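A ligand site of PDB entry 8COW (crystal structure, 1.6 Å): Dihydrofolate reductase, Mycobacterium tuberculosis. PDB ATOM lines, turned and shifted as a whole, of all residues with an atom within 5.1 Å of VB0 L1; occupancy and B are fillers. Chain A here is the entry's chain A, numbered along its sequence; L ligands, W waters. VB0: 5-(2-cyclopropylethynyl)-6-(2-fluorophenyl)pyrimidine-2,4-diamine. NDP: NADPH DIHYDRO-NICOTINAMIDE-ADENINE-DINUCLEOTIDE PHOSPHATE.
Water W2 lies within hydrogen-bond range of N04 of VB0 L1 (2.9 Å), OG1 of Thr 115 (2.9 Å), O of Glu 113 (3.0 Å), ND1 of His 32 (3.3 Å) and O of Trp 8 (3.4 Å).
Merely in contact with VB0 L1: Phe 33 (2.9 Å), Leu 52 (3.6 Å), Ile 22 (3.6 Å), Thr 115 (3.7 Å), Ala 9 (3.7 Å), Thr 48 (3.8 Å) and Gln 30 (3.9 Å).
Hydrophobic or aromatic side chains that line VB0 L1: Ile 7, Ala 9, Ile 22, Phe 33, Leu 52 and Ile 96.
Of the 17 residues printed, 12 come within 4 Å of VB0 L1.
The nearest printed residue that does not touch VB0 L1 is His 32 (4.5 Å).
A nitrogen (N03) of VB0 L1 sits at hydrogen-bond distance from the backbone carbonyl oxygen (O) of Ile 7 (2.9 Å).
A nitrogen (N03) of VB0 L1 lies within hydrogen-bond range of the backbone carbonyl oxygen of Ile 96, at 3.0 Å.
The side-chain hydroxyl of Thr 48 lies within hydrogen-bond range of an oxygen (O1A) of NDP L2 (2.7 Å).
A nitrogen (N04) of VB0 L1 sits at hydrogen-bond distance from the side-chain carboxylate (OD1) of Asp 29, 2.7 Å away.
The side-chain hydroxyl of Tyr 102 sits at hydrogen-bond distance from a nitrogen (N03) of VB0 L1 (3.3 Å).
A nitrogen (N04) of VB0 L1 sits at hydrogen-bond distance from the backbone carbonyl oxygen (O) of Trp 8 (3.5 Å).
The backbone NH (N) of Thr 48 is in hydrogen-bond range of an oxygen (O1A) of NDP L2 (3.2 Å).
OH of Tyr 102 lies within hydrogen-bond range of O of Ile 7 (2.6 Å).
OG of Ser 51 lies within hydrogen-bond range of O of Thr 48 (2.6 Å).
The side-chain carboxylate (OD1) of Asp 29 is in hydrogen-bond range of the side-chain hydroxyl (OG1) of Thr 115 (2.6 Å).
O of Trp 8 sits at hydrogen-bond distance from N of Thr 115.
The backbone NH of Trp 8 sits at hydrogen-bond distance from the backbone carbonyl oxygen of Glu 113 (3.2 Å).
The backbone carbonyl oxygen of Ile 96 sits at hydrogen-bond distance from the side-chain hydroxyl of Tyr 102 (3.1 Å).
The side-chain hydroxyl (OH) of Tyr 102 sits close to the backbone NH (N) of Gly 97 (3.4 Å).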
ATOM      1  N   ILE A   7       9.058   9.933   0.261  1.00  0.00           N
ATOM      2  CA  ILE A   7      10.035   9.953   1.342  1.00  0.00           C
ATOM      3  C   ILE A   7      10.852  11.242   1.231  1.00  0.00           C
ATOM      4  O   ILE A   7      11.375  11.563   0.146  1.00  0.00           O
ATOM      5  CB  ILE A   7      10.926   8.688   1.319  1.00  0.00           C
ATOM      6  CG1 ILE A   7      11.886   8.646   2.515  1.00  0.00           C
ATOM      7  CG2 ILE A   7      11.695   8.550  -0.005  1.00  0.00           C
ATOM      8  CD1 ILE A   7      12.327   7.197   2.885  1.00  0.00           C
ATOM      9  N   TRP A   8      10.964  11.983   2.327  1.00  0.00           N
ATOM     10  CA  TRP A   8      11.783  13.195   2.327  1.00  0.00           C
ATOM     11  C   TRP A   8      12.300  13.494   3.726  1.00  0.00           C
ATOM     12  O   TRP A   8      11.782  12.991   4.726  1.00  0.00           O
ATOM     13  CB  TRP A   8      10.992  14.400   1.793  1.00  0.00           C
ATOM     14  CG  TRP A   8       9.923  14.938   2.698  1.00  0.00           C
ATOM     15  CD1 TRP A   8      10.079  15.774   3.770  1.00  0.00           C
ATOM     16  CD2 TRP A   8       8.519  14.706   2.567  1.00  0.00           C
ATOM     17  NE1 TRP A   8       8.846  16.068   4.305  1.00  0.00           N
ATOM     18  CE2 TRP A   8       7.872  15.422   3.592  1.00  0.00           C
ATOM     19  CE3 TRP A   8       7.748  13.940   1.681  1.00  0.00           C
ATOM     20  CZ2 TRP A   8       6.491  15.402   3.757  1.00  0.00           C
ATOM     21  CZ3 TRP A   8       6.377  13.931   1.847  1.00  0.00           C
ATOM     22  CH2 TRP A   8       5.762  14.665   2.873  1.00  0.00           C
ATOM     23  N   ALA A   9      13.319  14.343   3.782  1.00  0.00           N
ATOM     24  CA  ALA A   9      13.836  14.871   5.033  1.00  0.00           C
ATOM     25  C   ALA A   9      13.727  16.388   4.982  1.00  0.00           C
ATOM     26  O   ALA A   9      14.175  17.012   4.019  1.00  0.00           O
ATOM     27  CB  ALA A   9      15.282  14.441   5.262  1.00  0.00           C
ATOM     28  N   ILE A  22      21.407  19.791  -0.213  1.00  0.00           N
ATOM     29  CA  ILE A  22      20.647  19.614   1.014  1.00  0.00           C
ATOM     30  C   ILE A  22      21.495  20.186   2.155  1.00  0.00           C
ATOM     31  O   ILE A  22      22.556  19.622   2.460  1.00  0.00           O
ATOM     32  CB  ILE A  22      20.261  18.148   1.248  1.00  0.00           C
ATOM     33  CG1 ILE A  22      19.371  17.666   0.116  1.00  0.00           C
ATOM     34  CG2 ILE A  22      19.521  17.960   2.590  1.00  0.00           C
ATOM     35  CD1 ILE A  22      19.153  16.156   0.097  1.00  0.00           C
ATOM     36  N   ASP A  29      19.583   9.453   8.722  1.00  0.00           N
ATOM     37  CA  ASP A  29      18.505   9.619   7.772  1.00  0.00           C
ATOM     38  C   ASP A  29      18.843   8.955   6.442  1.00  0.00           C
ATOM     39  O   ASP A  29      17.975   8.351   5.794  1.00  0.00           O
ATOM     40  CB  ASP A  29      18.217  11.101   7.544  1.00  0.00           C
ATOM     41  CG  ASP A  29      17.257  11.326   6.392  1.00  0.00           C
ATOM     42  OD1 ASP A  29      16.063  10.916   6.517  1.00  0.00           O
ATOM     43  OD2 ASP A  29      17.715  11.839   5.332  1.00  0.00           O
ATOM     44  N   GLN A  30      20.091   9.067   6.011  1.00  0.00           N
ATOM     45  CA  GLN A  30      20.540   8.371   4.800  1.00  0.00           C
ATOM     46  C   GLN A  30      20.371   6.869   4.937  1.00  0.00           C
ATOM     47  O   GLN A  30      19.883   6.211   4.005  1.00  0.00           O
ATOM     48  CB  GLN A  30      21.993   8.733   4.503  1.00  0.00           C
ATOM     49  CG  GLN A  30      22.526   8.104   3.204  1.00  0.00           C
ATOM     50  CD  GLN A  30      23.887   8.640   2.803  1.00  0.00           C
ATOM     51  OE1 GLN A  30      24.241   9.770   3.130  1.00  0.00           O
ATOM     52  NE2 GLN A  30      24.684   7.808   2.133  1.00  0.00           N
ATOM     53  N   HIS A  32      18.268   5.342   6.906  1.00  0.00           N
ATOM     54  CA  HIS A  32      16.824   5.185   6.839  1.00  0.00           C
ATOM     55  C   HIS A  32      16.331   5.205   5.401  1.00  0.00           C
ATOM     56  O   HIS A  32      15.532   4.361   4.985  1.00  0.00           O
ATOM     57  CB  HIS A  32      16.153   6.294   7.675  1.00  0.00           C
ATOM     58  CG  HIS A  32      14.656   6.309   7.641  1.00  0.00           C
ATOM     59  ND1 HIS A  32      13.951   7.309   7.022  1.00  0.00           N
ATOM     60  CD2 HIS A  32      13.740   5.464   8.176  1.00  0.00           C
ATOM     61  CE1 HIS A  32      12.656   7.087   7.173  1.00  0.00           C
ATOM     62  NE2 HIS A  32      12.502   5.967   7.858  1.00  0.00           N
ATOM     63  N   PHE A  33      16.775   6.206   4.632  1.00  0.00           N
ATOM     64  CA  PHE A  33      16.356   6.335   3.247  1.00  0.00           C
ATOM     65  C   PHE A  33      16.781   5.127   2.438  1.00  0.00           C
ATOM     66  O   PHE A  33      16.038   4.632   1.577  1.00  0.00           O
ATOM     67  CB  PHE A  33      16.944   7.624   2.668  1.00  0.00           C
ATOM     68  CG  PHE A  33      16.844   7.724   1.181  1.00  0.00           C
ATOM     69  CD1 PHE A  33      17.901   7.328   0.367  1.00  0.00           C
ATOM     70  CD2 PHE A  33      15.702   8.200   0.581  1.00  0.00           C
ATOM     71  CE1 PHE A  33      17.809   7.428  -1.009  1.00  0.00           C
ATOM     72  CE2 PHE A  33      15.587   8.292  -0.795  1.00  0.00           C
ATOM     73  CZ  PHE A  33      16.647   7.899  -1.580  1.00  0.00           C
ATOM     74  N   THR A  48      16.883  16.943  -9.135  1.00  0.00           N
ATOM     75  CA  THR A  48      17.440  16.077  -8.111  1.00  0.00           C
ATOM     76  C   THR A  48      18.429  15.084  -8.714  1.00  0.00           C
ATOM     77  O   THR A  48      19.501  14.839  -8.148  1.00  0.00           O
ATOM     78  CB  THR A  48      16.321  15.376  -7.360  1.00  0.00           C
ATOM     79  OG1 THR A  48      15.593  16.355  -6.608  1.00  0.00           O
ATOM     80  CG2 THR A  48      16.882  14.353  -6.392  1.00  0.00           C
ATOM     81  N   SER A  51      21.580  16.797  -9.145  1.00  0.00           N
ATOM     82  CA  SER A  51      22.303  17.064  -7.900  1.00  0.00           C
ATOM     83  C   SER A  51      23.127  15.866  -7.432  1.00  0.00           C
ATOM     84  O   SER A  51      23.973  16.035  -6.534  1.00  0.00           O
ATOM     85  CB  SER A  51      21.328  17.473  -6.785  1.00  0.00           C
ATOM     86  OG  SER A  51      20.579  16.368  -6.289  1.00  0.00           O
ATOM     87  N   LEU A  52      22.934  14.687  -8.001  1.00  0.00           N
ATOM     88  CA  LEU A  52      23.777  13.554  -7.618  1.00  0.00           C
ATOM     89  C   LEU A  52      25.062  13.550  -8.430  1.00  0.00           C
ATOM     90  O   LEU A  52      25.006  13.587  -9.659  1.00  0.00           O
ATOM     91  CB  LEU A  52      23.046  12.231  -7.825  1.00  0.00           C
ATOM     92  CG  LEU A  52      21.674  12.101  -7.179  1.00  0.00           C
ATOM     93  CD1 LEU A  52      20.941  10.854  -7.673  1.00  0.00           C
ATOM     94  CD2 LEU A  52      21.913  12.014  -5.698  1.00  0.00           C
ATOM     95  N   LEU A  59      21.349   5.271  -8.083  1.00  0.00           N
ATOM     96  CA  LEU A  59      21.446   4.723  -6.752  1.00  0.00           C
ATOM     97  C   LEU A  59      21.394   3.208  -6.844  1.00  0.00           C
ATOM     98  O   LEU A  59      20.507   2.671  -7.523  1.00  0.00           O
ATOM     99  CB  LEU A  59      20.317   5.258  -5.868  1.00  0.00           C
ATOM    100  CG  LEU A  59      20.326   6.770  -5.663  1.00  0.00           C
ATOM    101  CD1 LEU A  59      19.164   7.146  -4.764  1.00  0.00           C
ATOM    102  CD2 LEU A  59      21.648   7.245  -5.096  1.00  0.00           C
ATOM    103  N   ILE A  96      11.292  10.261  -4.456  1.00  0.00           N
ATOM    104  CA  ILE A  96      12.404  10.643  -3.582  1.00  0.00           C
ATOM    105  C   ILE A  96      12.822  12.104  -3.755  1.00  0.00           C
ATOM    106  O   ILE A  96      13.868  12.500  -3.215  1.00  0.00           O
ATOM    107  CB  ILE A  96      13.607   9.704  -3.750  1.00  0.00           C
ATOM    108  CG1 ILE A  96      14.284   9.874  -5.120  1.00  0.00           C
ATOM    109  CG2 ILE A  96      13.155   8.242  -3.547  1.00  0.00           C
ATOM    110  CD1 ILE A  96      15.717   9.337  -5.203  1.00  0.00           C
ATOM    111  N   GLY A  97      12.049  12.918  -4.461  1.00  0.00           N
ATOM    112  CA  GLY A  97      12.283  14.348  -4.524  1.00  0.00           C
ATOM    113  C   GLY A  97      12.442  14.837  -5.963  1.00  0.00           C
ATOM    114  O   GLY A  97      12.492  14.054  -6.904  1.00  0.00           O
ATOM    115  N   TYR A 102       7.434  16.068  -5.454  1.00  0.00           N
ATOM    116  CA  TYR A 102       6.579  15.682  -4.321  1.00  0.00           C
ATOM    117  C   TYR A 102       5.174  16.239  -4.494  1.00  0.00           C
ATOM    118  O   TYR A 102       4.180  15.551  -4.220  1.00  0.00           O
ATOM    119  CB  TYR A 102       7.154  16.221  -3.014  1.00  0.00           C
ATOM    120  CG  TYR A 102       8.390  15.553  -2.515  1.00  0.00           C
ATOM    121  CD1 TYR A 102       8.533  14.173  -2.540  1.00  0.00           C
ATOM    122  CD2 TYR A 102       9.446  16.309  -2.024  1.00  0.00           C
ATOM    123  CE1 TYR A 102       9.721  13.569  -2.082  1.00  0.00           C
ATOM    124  CE2 TYR A 102      10.628  15.710  -1.560  1.00  0.00           C
ATOM    125  CZ  TYR A 102      10.750  14.339  -1.594  1.00  0.00           C
ATOM    126  OH  TYR A 102      11.935  13.766  -1.144  1.00  0.00           O
ATOM    127  N   GLU A 113       6.951   8.960   4.340  1.00  0.00           N
ATOM    128  CA  GLU A 113       7.915   8.678   5.384  1.00  0.00           C
ATOM    129  C   GLU A 113       8.774   9.935   5.523  1.00  0.00           C
ATOM    130  O   GLU A 113       9.531  10.282   4.612  1.00  0.00           O
ATOM    131  CB  GLU A 113       8.767   7.448   5.053  1.00  0.00           C
ATOM    132  CG  GLU A 113       7.955   6.144   5.075  1.00  0.00           C
ATOM    133  CD  GLU A 113       7.538   5.711   6.488  1.00  0.00           C
ATOM    134  OE1 GLU A 113       6.576   4.908   6.599  1.00  0.00           O
ATOM    135  OE2 GLU A 113       8.139   6.163   7.491  1.00  0.00           O
ATOM    136  N   THR A 115      11.360  12.582   7.661  1.00  0.00           N
ATOM    137  CA  THR A 115      12.353  12.884   8.675  1.00  0.00           C
ATOM    138  C   THR A 115      12.279  14.373   8.986  1.00  0.00           C
ATOM    139  O   THR A 115      12.440  15.209   8.091  1.00  0.00           O
ATOM    140  CB  THR A 115      13.764  12.516   8.197  1.00  0.00           C
ATOM    141  OG1 THR A 115      13.824  11.101   7.915  1.00  0.00           O
ATOM    142  CG2 THR A 115      14.783  12.856   9.268  1.00  0.00           C
HETATM  143  C10 VB0 L   1      19.059  13.269   2.301  1.00  0.00           C
HETATM  144  C13 VB0 L   1      17.882  12.529  -3.242  1.00  0.00           C
HETATM  145  C15 VB0 L   1      18.923  11.535  -3.724  1.00  0.00           C
HETATM  146  C01 VB0 L   1      15.129  11.167   3.044  1.00  0.00           C
HETATM  147  C02 VB0 L   1      17.121  11.708   1.829  1.00  0.00           C
HETATM  148  C03 VB0 L   1      16.361  11.737   0.640  1.00  0.00           C
HETATM  149  C04 VB0 L   1      15.017  11.444   0.794  1.00  0.00           C
HETATM  150  C05 VB0 L   1      18.633  12.001   1.912  1.00  0.00           C
HETATM  151  C06 VB0 L   1      19.560  11.012   1.622  1.00  0.00           C
HETATM  152  C07 VB0 L   1      20.926  11.291   1.704  1.00  0.00           C
HETATM  153  C08 VB0 L   1      21.345  12.566   2.083  1.00  0.00           C
HETATM  154  C09 VB0 L   1      20.412  13.559   2.379  1.00  0.00           C
HETATM  155  C11 VB0 L   1      16.957  12.022  -0.728  1.00  0.00           C
HETATM  156  C12 VB0 L   1      17.354  12.247  -1.831  1.00  0.00           C
HETATM  157  C14 VB0 L   1      19.353  12.925  -3.277  1.00  0.00           C
HETATM  158  F01 VB0 L   1      19.139   9.765   1.253  1.00  0.00           F
HETATM  159  N01 VB0 L   1      14.398  11.173   1.925  1.00  0.00           N
HETATM  160  N02 VB0 L   1      16.428  11.439   2.924  1.00  0.00           N
HETATM  161  N03 VB0 L   1      14.193  11.444  -0.402  1.00  0.00           N
HETATM  162  N04 VB0 L   1      14.514  10.860   4.321  1.00  0.00           N
HETATM  163  PA  NDP L   2      12.881  18.589  -8.682  1.00  0.00           P
HETATM  164  O1A NDP L   2      13.862  17.653  -8.173  1.00  0.00           O
HETATM  165  O2A NDP L   2      11.516  18.440  -8.285  1.00  0.00           O
HETATM  166  O5B NDP L   2      12.980  18.592 -10.257  1.00  0.00           O
HETATM  167  C5B NDP L   2      12.254  19.527 -11.001  1.00  0.00           C
HETATM  168  C4B NDP L   2      12.232  19.071 -12.441  1.00  0.00           C
HETATM  169  O4B NDP L   2      11.380  17.939 -12.597  1.00  0.00           O
HETATM  170  C3B NDP L   2      11.714  20.071 -13.460  1.00  0.00           C
HETATM  171  O3B NDP L   2      12.700  21.045 -13.735  1.00  0.00           O
HETATM  172  C2B NDP L   2      11.413  19.143 -14.614  1.00  0.00           C
HETATM  173  O2B NDP L   2      12.597  18.829 -15.283  1.00  0.00           O
HETATM  174  C1B NDP L   2      10.844  17.934 -13.879  1.00  0.00           C
HETATM  175  N9A NDP L   2       9.405  17.969 -13.755  1.00  0.00           N
HETATM  176  C8A NDP L   2       8.718  18.772 -12.897  1.00  0.00           C
HETATM  177  N7A NDP L   2       7.435  18.649 -13.008  1.00  0.00           N
HETATM  178  C5A NDP L   2       7.248  17.730 -14.008  1.00  0.00           C
HETATM  179  C6A NDP L   2       6.094  17.200 -14.614  1.00  0.00           C
HETATM  180  N6A NDP L   2       4.873  17.559 -14.276  1.00  0.00           N
HETATM  181  N1A NDP L   2       6.256  16.288 -15.596  1.00  0.00           N
HETATM  182  C2A NDP L   2       7.488  15.948 -15.939  1.00  0.00           C
HETATM  183  N3A NDP L   2       8.639  16.391 -15.455  1.00  0.00           N
HETATM  184  C4A NDP L   2       8.461  17.298 -14.485  1.00  0.00           C
HETATM  185  O3  NDP L   2      13.267  20.064  -8.344  1.00  0.00           O
HETATM  186  PN  NDP L   2      13.189  20.936  -7.027  1.00  0.00           P
HETATM  187  O1N NDP L   2      13.960  22.125  -7.320  1.00  0.00           O
HETATM  188  O2N NDP L   2      11.812  21.124  -6.623  1.00  0.00           O
HETATM  189  O5D NDP L   2      13.960  20.114  -5.932  1.00  0.00           O
HETATM  190  C5D NDP L   2      15.370  19.991  -5.949  1.00  0.00           C
HETATM  191  C4D NDP L   2      15.964  20.256  -4.593  1.00  0.00           C
HETATM  192  O4D NDP L   2      15.452  19.373  -3.576  1.00  0.00           O
HETATM  193  C3D NDP L   2      17.482  20.123  -4.495  1.00  0.00           C
HETATM  194  O3D NDP L   2      17.963  21.141  -3.641  1.00  0.00           O
HETATM  195  C2D NDP L   2      17.631  18.775  -3.839  1.00  0.00           C
HETATM  196  O2D NDP L   2      18.818  18.679  -3.135  1.00  0.00           O
HETATM  197  C1D NDP L   2      16.495  18.822  -2.865  1.00  0.00           C
HETATM  198  N1N NDP L   2      16.113  17.480  -2.397  1.00  0.00           N
HETATM  199  C2N NDP L   2      16.002  17.231  -1.072  1.00  0.00           C
HETATM  200  C3N NDP L   2      15.487  16.115  -0.602  1.00  0.00           C
HETATM  201  C7N NDP L   2      15.305  15.954   0.827  1.00  0.00           C
HETATM  202  O7N NDP L   2      15.712  16.779   1.622  1.00  0.00           O
HETATM  203  N7N NDP L   2      14.704  14.849   1.169  1.00  0.00           N
HETATM  204  C4N NDP L   2      15.137  15.056  -1.520  1.00  0.00           C
HETATM  205  C5N NDP L   2      15.437  15.345  -2.913  1.00  0.00           C
HETATM  206  C6N NDP L   2      15.895  16.501  -3.282  1.00  0.00           C
HETATM  207  P2B NDP L   2      13.078  19.557 -16.641  1.00  0.00           P
HETATM  208  O1X NDP L   2      13.395  20.862 -16.252  1.00  0.00           O
HETATM  209  O2X NDP L   2      11.985  19.496 -17.529  1.00  0.00           O
HETATM  210  O3X NDP L   2      14.180  18.817 -17.103  1.00  0.00           O
HETATM  211  O   HOH W   1      19.525  13.673   5.661  1.00  0.00           O
HETATM  212  O   HOH W   2      12.212   9.840   5.799  1.00  0.00           O
